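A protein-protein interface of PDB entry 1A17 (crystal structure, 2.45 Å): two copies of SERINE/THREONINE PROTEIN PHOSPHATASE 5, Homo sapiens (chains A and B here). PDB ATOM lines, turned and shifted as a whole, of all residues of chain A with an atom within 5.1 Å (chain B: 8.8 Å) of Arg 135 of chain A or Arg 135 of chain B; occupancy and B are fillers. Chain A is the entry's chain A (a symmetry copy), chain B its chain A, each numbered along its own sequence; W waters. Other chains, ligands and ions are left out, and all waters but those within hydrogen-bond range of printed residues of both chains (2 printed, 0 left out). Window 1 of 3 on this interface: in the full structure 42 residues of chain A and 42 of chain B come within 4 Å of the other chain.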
ATOM      1  N   GLN A 130     -41.669  18.193  26.487  1.00  0.00           N
ATOM      2  CA  GLN A 130     -40.886  18.136  27.746  1.00  0.00           C
ATOM      3  C   GLN A 130     -39.438  17.775  27.426  1.00  0.00           C
ATOM      4  O   GLN A 130     -38.530  18.114  28.180  1.00  0.00           O
ATOM      5  CB  GLN A 130     -41.428  17.087  28.743  1.00  0.00           C
ATOM      6  CG  GLN A 130     -42.751  17.421  29.449  1.00  0.00           C
ATOM      7  CD  GLN A 130     -43.367  16.250  30.256  1.00  0.00           C
ATOM      8  OE1 GLN A 130     -42.903  15.106  30.202  1.00  0.00           O
ATOM      9  NE2 GLN A 130     -44.423  16.544  30.987  1.00  0.00           N
ATOM     10  N   LYS A 131     -39.229  17.033  26.337  1.00  0.00           N
ATOM     11  CA  LYS A 131     -37.889  16.624  25.910  1.00  0.00           C
ATOM     12  C   LYS A 131     -37.112  17.814  25.372  1.00  0.00           C
ATOM     13  O   LYS A 131     -35.940  17.983  25.662  1.00  0.00           O
ATOM     14  CB  LYS A 131     -37.965  15.553  24.831  1.00  0.00           C
ATOM     15  CG  LYS A 131     -36.607  15.014  24.429  1.00  0.00           C
ATOM     16  CD  LYS A 131     -36.724  14.179  23.186  1.00  0.00           C
ATOM     17  CE  LYS A 131     -35.397  13.554  22.832  1.00  0.00           C
ATOM     18  NZ  LYS A 131     -35.535  12.322  21.997  1.00  0.00           N
ATOM     19  N   ALA A 132     -37.766  18.629  24.566  1.00  0.00           N
ATOM     20  CA  ALA A 132     -37.128  19.810  24.028  1.00  0.00           C
ATOM     21  C   ALA A 132     -36.874  20.744  25.208  1.00  0.00           C
ATOM     22  O   ALA A 132     -35.926  21.518  25.186  1.00  0.00           O
ATOM     23  CB  ALA A 132     -38.030  20.472  23.016  1.00  0.00           C
ATOM     24  N   PHE A 133     -37.711  20.634  26.245  1.00  0.00           N
ATOM     25  CA  PHE A 133     -37.600  21.439  27.470  1.00  0.00           C
ATOM     26  C   PHE A 133     -36.352  21.097  28.304  1.00  0.00           C
ATOM     27  O   PHE A 133     -35.507  21.946  28.528  1.00  0.00           O
ATOM     28  CB  PHE A 133     -38.878  21.291  28.333  1.00  0.00           C
ATOM     29  CG  PHE A 133     -38.969  22.301  29.472  1.00  0.00           C
ATOM     30  CD1 PHE A 133     -38.423  22.026  30.720  1.00  0.00           C
ATOM     31  CD2 PHE A 133     -39.601  23.521  29.286  1.00  0.00           C
ATOM     32  CE1 PHE A 133     -38.492  22.965  31.749  1.00  0.00           C
ATOM     33  CE2 PHE A 133     -39.674  24.461  30.306  1.00  0.00           C
ATOM     34  CZ  PHE A 133     -39.130  24.185  31.535  1.00  0.00           C
ATOM     35  N   GLU A 134     -36.261  19.866  28.776  1.00  0.00           N
ATOM     36  CA  GLU A 134     -35.128  19.392  29.565  1.00  0.00           C
ATOM     37  C   GLU A 134     -33.811  19.656  28.833  1.00  0.00           C
ATOM     38  O   GLU A 134     -32.772  19.834  29.479  1.00  0.00           O
ATOM     39  CB  GLU A 134     -35.235  17.878  29.773  1.00  0.00           C
ATOM     40  CG  GLU A 134     -36.594  17.363  30.206  1.00  0.00           C
ATOM     41  CD  GLU A 134     -36.843  17.490  31.679  1.00  0.00           C
ATOM     42  OE1 GLU A 134     -36.063  18.185  32.370  1.00  0.00           O
ATOM     43  OE2 GLU A 134     -37.832  16.881  32.149  1.00  0.00           O
ATOM     44  N   ARG A 135     -33.840  19.601  27.498  1.00  0.00           N
ATOM     45  CA  ARG A 135     -32.650  19.843  26.683  1.00  0.00           C
ATOM     46  C   ARG A 135     -32.246  21.315  26.693  1.00  0.00           C
ATOM     47  O   ARG A 135     -31.074  21.655  26.806  1.00  0.00           O
ATOM     48  CB  ARG A 135     -32.876  19.364  25.243  1.00  0.00           C
ATOM     49  CG  ARG A 135     -32.670  17.846  25.050  1.00  0.00           C
ATOM     50  CD  ARG A 135     -33.032  17.341  23.648  1.00  0.00           C
ATOM     51  NE  ARG A 135     -32.193  17.885  22.586  1.00  0.00           N
ATOM     52  CZ  ARG A 135     -31.168  17.248  22.026  1.00  0.00           C
ATOM     53  NH1 ARG A 135     -30.834  16.033  22.424  1.00  0.00           N
ATOM     54  NH2 ARG A 135     -30.498  17.819  21.034  1.00  0.00           N
ATOM     55  N   ALA A 136     -33.227  22.197  26.621  1.00  0.00           N
ATOM     56  CA  ALA A 136     -32.979  23.628  26.637  1.00  0.00           C
ATOM     57  C   ALA A 136     -32.369  24.050  27.969  1.00  0.00           C
ATOM     58  O   ALA A 136     -31.348  24.737  28.013  1.00  0.00           O
ATOM     59  CB  ALA A 136     -34.279  24.370  26.386  1.00  0.00           C
ATOM     60  N   ILE A 137     -33.002  23.628  29.055  1.00  0.00           N
ATOM     61  CA  ILE A 137     -32.525  23.924  30.390  1.00  0.00           C
ATOM     62  C   ILE A 137     -31.057  23.530  30.521  1.00  0.00           C
ATOM     63  O   ILE A 137     -30.222  24.336  30.926  1.00  0.00           O
ATOM     64  CB  ILE A 137     -33.340  23.151  31.422  1.00  0.00           C
ATOM     65  CG1 ILE A 137     -34.784  23.615  31.398  1.00  0.00           C
ATOM     66  CG2 ILE A 137     -32.783  23.369  32.793  1.00  0.00           C
ATOM     67  CD1 ILE A 137     -34.965  25.026  31.907  1.00  0.00           C
ATOM     68  N   ALA A 138     -30.743  22.297  30.152  1.00  0.00           N
ATOM     69  CA  ALA A 138     -29.374  21.790  30.232  1.00  0.00           C
ATOM     70  C   ALA A 138     -28.437  22.695  29.444  1.00  0.00           C
ATOM     71  O   ALA A 138     -27.293  22.920  29.837  1.00  0.00           O
ATOM     72  CB  ALA A 138     -29.317  20.368  29.702  1.00  0.00           C
ATOM     73  N   GLY A 139     -28.920  23.197  28.321  1.00  0.00           N
ATOM     74  CA  GLY A 139     -28.129  24.104  27.510  1.00  0.00           C
ATOM     75  C   GLY A 139     -28.010  25.460  28.199  1.00  0.00           C
ATOM     76  O   GLY A 139     -27.016  26.168  28.021  1.00  0.00           O
ATOM     77  N   VAL B 128     -18.375  23.921  22.372  1.00  0.00           N
ATOM     78  CA  VAL B 128     -19.466  23.680  21.432  1.00  0.00           C
ATOM     79  C   VAL B 128     -19.864  22.200  21.503  1.00  0.00           C
ATOM     80  O   VAL B 128     -21.055  21.856  21.390  1.00  0.00           O
ATOM     81  CB  VAL B 128     -19.036  23.994  19.991  1.00  0.00           C
ATOM     82  CG1 VAL B 128     -20.122  23.619  19.021  1.00  0.00           C
ATOM     83  CG2 VAL B 128     -18.705  25.454  19.861  1.00  0.00           C
ATOM     84  N   LYS B 129     -18.868  21.336  21.706  1.00  0.00           N
ATOM     85  CA  LYS B 129     -19.092  19.903  21.805  1.00  0.00           C
ATOM     86  C   LYS B 129     -19.633  19.488  23.169  1.00  0.00           C
ATOM     87  O   LYS B 129     -20.462  18.585  23.223  1.00  0.00           O
ATOM     88  CB  LYS B 129     -17.834  19.126  21.419  1.00  0.00           C
ATOM     89  CG  LYS B 129     -17.565  19.142  19.886  1.00  0.00           C
ATOM     90  CD  LYS B 129     -16.177  18.576  19.474  1.00  0.00           C
ATOM     91  CE  LYS B 129     -16.002  18.545  17.937  1.00  0.00           C
ATOM     92  NZ  LYS B 129     -14.661  18.060  17.459  1.00  0.00           N
ATOM     93  N   GLN B 130     -19.222  20.173  24.255  1.00  0.00           N
ATOM     94  CA  GLN B 130     -19.714  19.885  25.625  1.00  0.00           C
ATOM     95  C   GLN B 130     -21.186  20.274  25.728  1.00  0.00           C
ATOM     96  O   GLN B 130     -21.919  19.728  26.548  1.00  0.00           O
ATOM     97  CB  GLN B 130     -18.940  20.659  26.716  1.00  0.00           C
ATOM     98  CG  GLN B 130     -17.506  20.194  27.010  1.00  0.00           C
ATOM     99  CD  GLN B 130     -16.698  21.136  27.937  1.00  0.00           C
ATOM    100  OE1 GLN B 130     -17.130  22.242  28.279  1.00  0.00           O
ATOM    101  NE2 GLN B 130     -15.517  20.695  28.324  1.00  0.00           N
ATOM    102  N   LYS B 131     -21.604  21.264  24.936  1.00  0.00           N
ATOM    103  CA  LYS B 131     -22.992  21.730  24.927  1.00  0.00           C
ATOM    104  C   LYS B 131     -23.901  20.696  24.284  1.00  0.00           C
ATOM    105  O   LYS B 131     -24.987  20.425  24.767  1.00  0.00           O
ATOM    106  CB  LYS B 131     -23.120  23.044  24.168  1.00  0.00           C
ATOM    107  CG  LYS B 131     -24.517  23.628  24.220  1.00  0.00           C
ATOM    108  CD  LYS B 131     -24.648  24.756  23.237  1.00  0.00           C
ATOM    109  CE  LYS B 131     -26.001  25.413  23.350  1.00  0.00           C
ATOM    110  NZ  LYS B 131     -26.012  26.821  22.847  1.00  0.00           N
ATOM    111  N   ALA B 132     -23.459  20.132  23.175  1.00  0.00           N
ATOM    112  CA  ALA B 132     -24.231  19.110  22.504  1.00  0.00           C
ATOM    113  C   ALA B 132     -24.251  17.899  23.432  1.00  0.00           C
ATOM    114  O   ALA B 132     -25.203  17.130  23.418  1.00  0.00           O
ATOM    115  CB  ALA B 132     -23.588  18.755  21.187  1.00  0.00           C
ATOM    116  N   PHE B 133     -23.208  17.764  24.257  1.00  0.00           N
ATOM    117  CA  PHE B 133     -23.074  16.670  25.230  1.00  0.00           C
ATOM    118  C   PHE B 133     -24.103  16.752  26.372  1.00  0.00           C
ATOM    119  O   PHE B 133     -24.903  15.850  26.548  1.00  0.00           O
ATOM    120  CB  PHE B 133     -21.637  16.629  25.805  1.00  0.00           C
ATOM    121  CG  PHE B 133     -21.331  15.364  26.600  1.00  0.00           C
ATOM    122  CD1 PHE B 133     -21.587  15.295  27.965  1.00  0.00           C
ATOM    123  CD2 PHE B 133     -20.789  14.251  25.977  1.00  0.00           C
ATOM    124  CE1 PHE B 133     -21.324  14.127  28.679  1.00  0.00           C
ATOM    125  CE2 PHE B 133     -20.524  13.084  26.683  1.00  0.00           C
ATOM    126  CZ  PHE B 133     -20.783  13.021  28.029  1.00  0.00           C
ATOM    127  N   GLU B 134     -24.055  17.819  27.152  1.00  0.00           N
ATOM    128  CA  GLU B 134     -24.977  18.043  28.261  1.00  0.00           C
ATOM    129  C   GLU B 134     -26.428  17.937  27.787  1.00  0.00           C
ATOM    130  O   GLU B 134     -27.307  17.570  28.574  1.00  0.00           O
ATOM    131  CB  GLU B 134     -24.785  19.456  28.820  1.00  0.00           C
ATOM    132  CG  GLU B 134     -23.350  19.881  29.067  1.00  0.00           C
ATOM    133  CD  GLU B 134     -22.793  19.389  30.369  1.00  0.00           C
ATOM    134  OE1 GLU B 134     -23.426  18.518  31.010  1.00  0.00           O
ATOM    135  OE2 GLU B 134     -21.709  19.885  30.754  1.00  0.00           O
ATOM    136  N   ARG B 135     -26.686  18.333  26.536  1.00  0.00           N
ATOM    137  CA  ARG B 135     -28.030  18.273  25.963  1.00  0.00           C
ATOM    138  C   ARG B 135     -28.464  16.836  25.684  1.00  0.00           C
ATOM    139  O   ARG B 135     -29.593  16.446  25.956  1.00  0.00           O
ATOM    140  CB  ARG B 135     -28.107  19.111  24.680  1.00  0.00           C
ATOM    141  CG  ARG B 135     -28.306  20.621  24.931  1.00  0.00           C
ATOM    142  CD  ARG B 135     -28.241  21.478  23.660  1.00  0.00           C
ATOM    143  NE  ARG B 135     -29.304  21.199  22.701  1.00  0.00           N
ATOM    144  CZ  ARG B 135     -30.408  21.929  22.557  1.00  0.00           C
ATOM    145  NH1 ARG B 135     -30.613  22.992  23.316  1.00  0.00           N
ATOM    146  NH2 ARG B 135     -31.292  21.612  21.622  1.00  0.00           N
ATOM    147  N   ALA B 136     -27.547  16.030  25.179  1.00  0.00           N
ATOM    148  CA  ALA B 136     -27.827  14.637  24.882  1.00  0.00           C
ATOM    149  C   ALA B 136     -28.146  13.871  26.161  1.00  0.00           C
ATOM    150  O   ALA B 136     -29.153  13.166  26.247  1.00  0.00           O
ATOM    151  CB  ALA B 136     -26.633  14.020  24.175  1.00  0.00           C
ATOM    152  N   ILE B 137     -27.282  14.020  27.155  1.00  0.00           N
ATOM    153  CA  ILE B 137     -27.468  13.378  28.440  1.00  0.00           C
ATOM    154  C   ILE B 137     -28.862  13.684  28.982  1.00  0.00           C
ATOM    155  O   ILE B 137     -29.612  12.778  29.337  1.00  0.00           O
ATOM    156  CB  ILE B 137     -26.429  13.885  29.435  1.00  0.00           C
ATOM    157  CG1 ILE B 137     -25.037  13.483  28.983  1.00  0.00           C
ATOM    158  CG2 ILE B 137     -26.682  13.308  30.792  1.00  0.00           C
ATOM    159  CD1 ILE B 137     -24.791  11.995  29.062  1.00  0.00           C
ATOM    160  N   ALA B 138     -29.213  14.961  29.017  1.00  0.00           N
ATOM    161  CA  ALA B 138     -30.517  15.391  29.517  1.00  0.00           C
ATOM    162  C   ALA B 138     -31.628  14.692  28.745  1.00  0.00           C
ATOM    163  O   ALA B 138     -32.666  14.341  29.305  1.00  0.00           O
ATOM    164  CB  ALA B 138     -30.647  16.900  29.393  1.00  0.00           C
ATOM    165  N   GLY B 139     -31.412  14.508  27.454  1.00  0.00           N
ATOM    166  CA  GLY B 139     -32.386  13.815  26.629  1.00  0.00           C
ATOM    167  C   GLY B 139     -32.391  12.325  26.957  1.00  0.00           C
ATOM    168  O   GLY B 139     -33.421  11.659  26.823  1.00  0.00           O
ATOM    169  N   ASP B 140     -31.242  11.810  27.390  1.00  0.00           N
ATOM    170  CA  ASP B 140     -31.097  10.413  27.758  1.00  0.00           C
ATOM    171  C   ASP B 140     -31.794  10.181  29.080  1.00  0.00           C
ATOM    172  O   ASP B 140     -32.504   9.190  29.266  1.00  0.00           O
ATOM    173  CB  ASP B 140     -29.634  10.085  27.961  1.00  0.00           C
ATOM    174  CG  ASP B 140     -28.876   9.866  26.665  1.00  0.00           C
ATOM    175  OD1 ASP B 140     -29.460   9.925  25.554  1.00  0.00           O
ATOM    176  OD2 ASP B 140     -27.660   9.605  26.771  1.00  0.00           O
ATOM    177  N   GLU B 141     -31.593  11.127  29.993  1.00  0.00           N
ATOM    178  CA  GLU B 141     -32.155  11.069  31.330  1.00  0.00           C
ATOM    179  C   GLU B 141     -33.657  11.147  31.278  1.00  0.00           C
ATOM    180  O   GLU B 141     -34.361  10.466  32.005  1.00  0.00           O
ATOM    181  CB  GLU B 141     -31.592  12.199  32.183  1.00  0.00           C
ATOM    182  CG  GLU B 141     -31.809  11.982  33.668  1.00  0.00           C
ATOM    183  CD  GLU B 141     -31.250  10.636  34.125  1.00  0.00           C
ATOM    184  OE1 GLU B 141     -29.997  10.502  34.146  1.00  0.00           O
ATOM    185  OE2 GLU B 141     -32.062   9.715  34.420  1.00  0.00           O
ATOM    186  N   HIS B 142     -34.152  11.995  30.408  1.00  0.00           N
ATOM    187  CA  HIS B 142     -35.579  12.130  30.246  1.00  0.00           C
ATOM    188  C   HIS B 142     -36.202  10.870  29.622  1.00  0.00           C
ATOM    189  O   HIS B 142     -37.320  10.511  29.957  1.00  0.00           O
ATOM    190  CB  HIS B 142     -35.878  13.347  29.366  1.00  0.00           C
ATOM    191  CG  HIS B 142     -37.318  13.483  28.995  1.00  0.00           C
ATOM    192  ND1 HIS B 142     -37.752  13.449  27.686  1.00  0.00           N
ATOM    193  CD2 HIS B 142     -38.410  13.707  29.754  1.00  0.00           C
ATOM    194  CE1 HIS B 142     -39.058  13.666  27.660  1.00  0.00           C
ATOM    195  NE2 HIS B 142     -39.477  13.819  28.903  1.00  0.00           N
HETATM  196  O   HOH W   1     -29.740  25.173  25.047  1.00  0.00           O
HETATM  197  O   HOH W   2     -31.375  13.458  23.687  1.00  0.00           O
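Gln 130 of chain A touches His 142 of chain B (CB to NE2, 3.8 Å). Lys 131 of chain A touches His 142 of chain B (CB to ND1, 3.6 Å). Glu 134 of chain A touches Ala 138 of chain B. Arg 135 of chain A touches Arg 135 of chain B (O to CG, 3.5 Å). CB of Ala 138 of chain A touches O of Glu 134 of chain B, 3.6 Å away. CB of Ala 138 of chain B touches CB of Ala 138 of chain A, at 3.7 Å.
Arg 135 of chain A touches just one residue of chain B: Arg 135. Arg 135 of chain B touches just one residue of chain A: Arg 135. No residue of chain B comes within 4 Å of Ala 136 of chain A. Of the printed residues of chain B, Lys 131 of chain A touches His 142. Printed residues of chain A within 4 Å of Ala 138 of chain B: Glu 134 and Ala 138. Of the printed residues of chain A, Glu 134 of chain B touches Ala 138 (3.6 Å). Of the printed residues of chain B, Gln 130 of chain A touches His 142. Of the printed residues of chain B, Ala 138 of chain A touches Glu 134 and Ala 138. Gly 139 of chain A touches none of the printed residues of chain B. The nearest residue of chain B that does not touch Arg 135 of chain A is Ala 136 of chain B (4.1 Å). The nearest printed residue of chain A that does not touch His 142 of chain B is Glu 134 of chain A (4.02 Å).
Hydrophobic or aromatic side chains of chain B within 4 Å of the printed part of chain A: Ala 138 and His 142. Of the 10 printed residues of chain A, 5 touch a printed residue of chain B. Among the printed residues, no Asp or Glu carboxylate lies within 4 Å of a Lys or Arg side-chain nitrogen of the other chain.
Water W1 bridges the guanidinium group (NH1) of Arg 135 of chain B and the backbone carbonyl oxygen (O) of Ala 136 of chain A. Water W2 lies within hydrogen-bond range of the guanidinium group (NH1) of Arg 135 of chain A (2.9 Å) and the backbone carbonyl oxygen (O) of Ala 136 of chain B (3.4 Å).
Glu 134 of chain A touches Ala 138 of chain B, and with the chains exchanged Ala 138 of chain A touches Glu 134 of chain B. Arg 135 of chain A touches its own counterpart, Arg 135 of chain B. Ala 138 of chain A touches its own counterpart, Ala 138 of chain B. 10 positions are printed for both chains. Of the 6 pairs that touch across the chains among the printed residues, 4 have their exchanged pair printed and touching as well.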
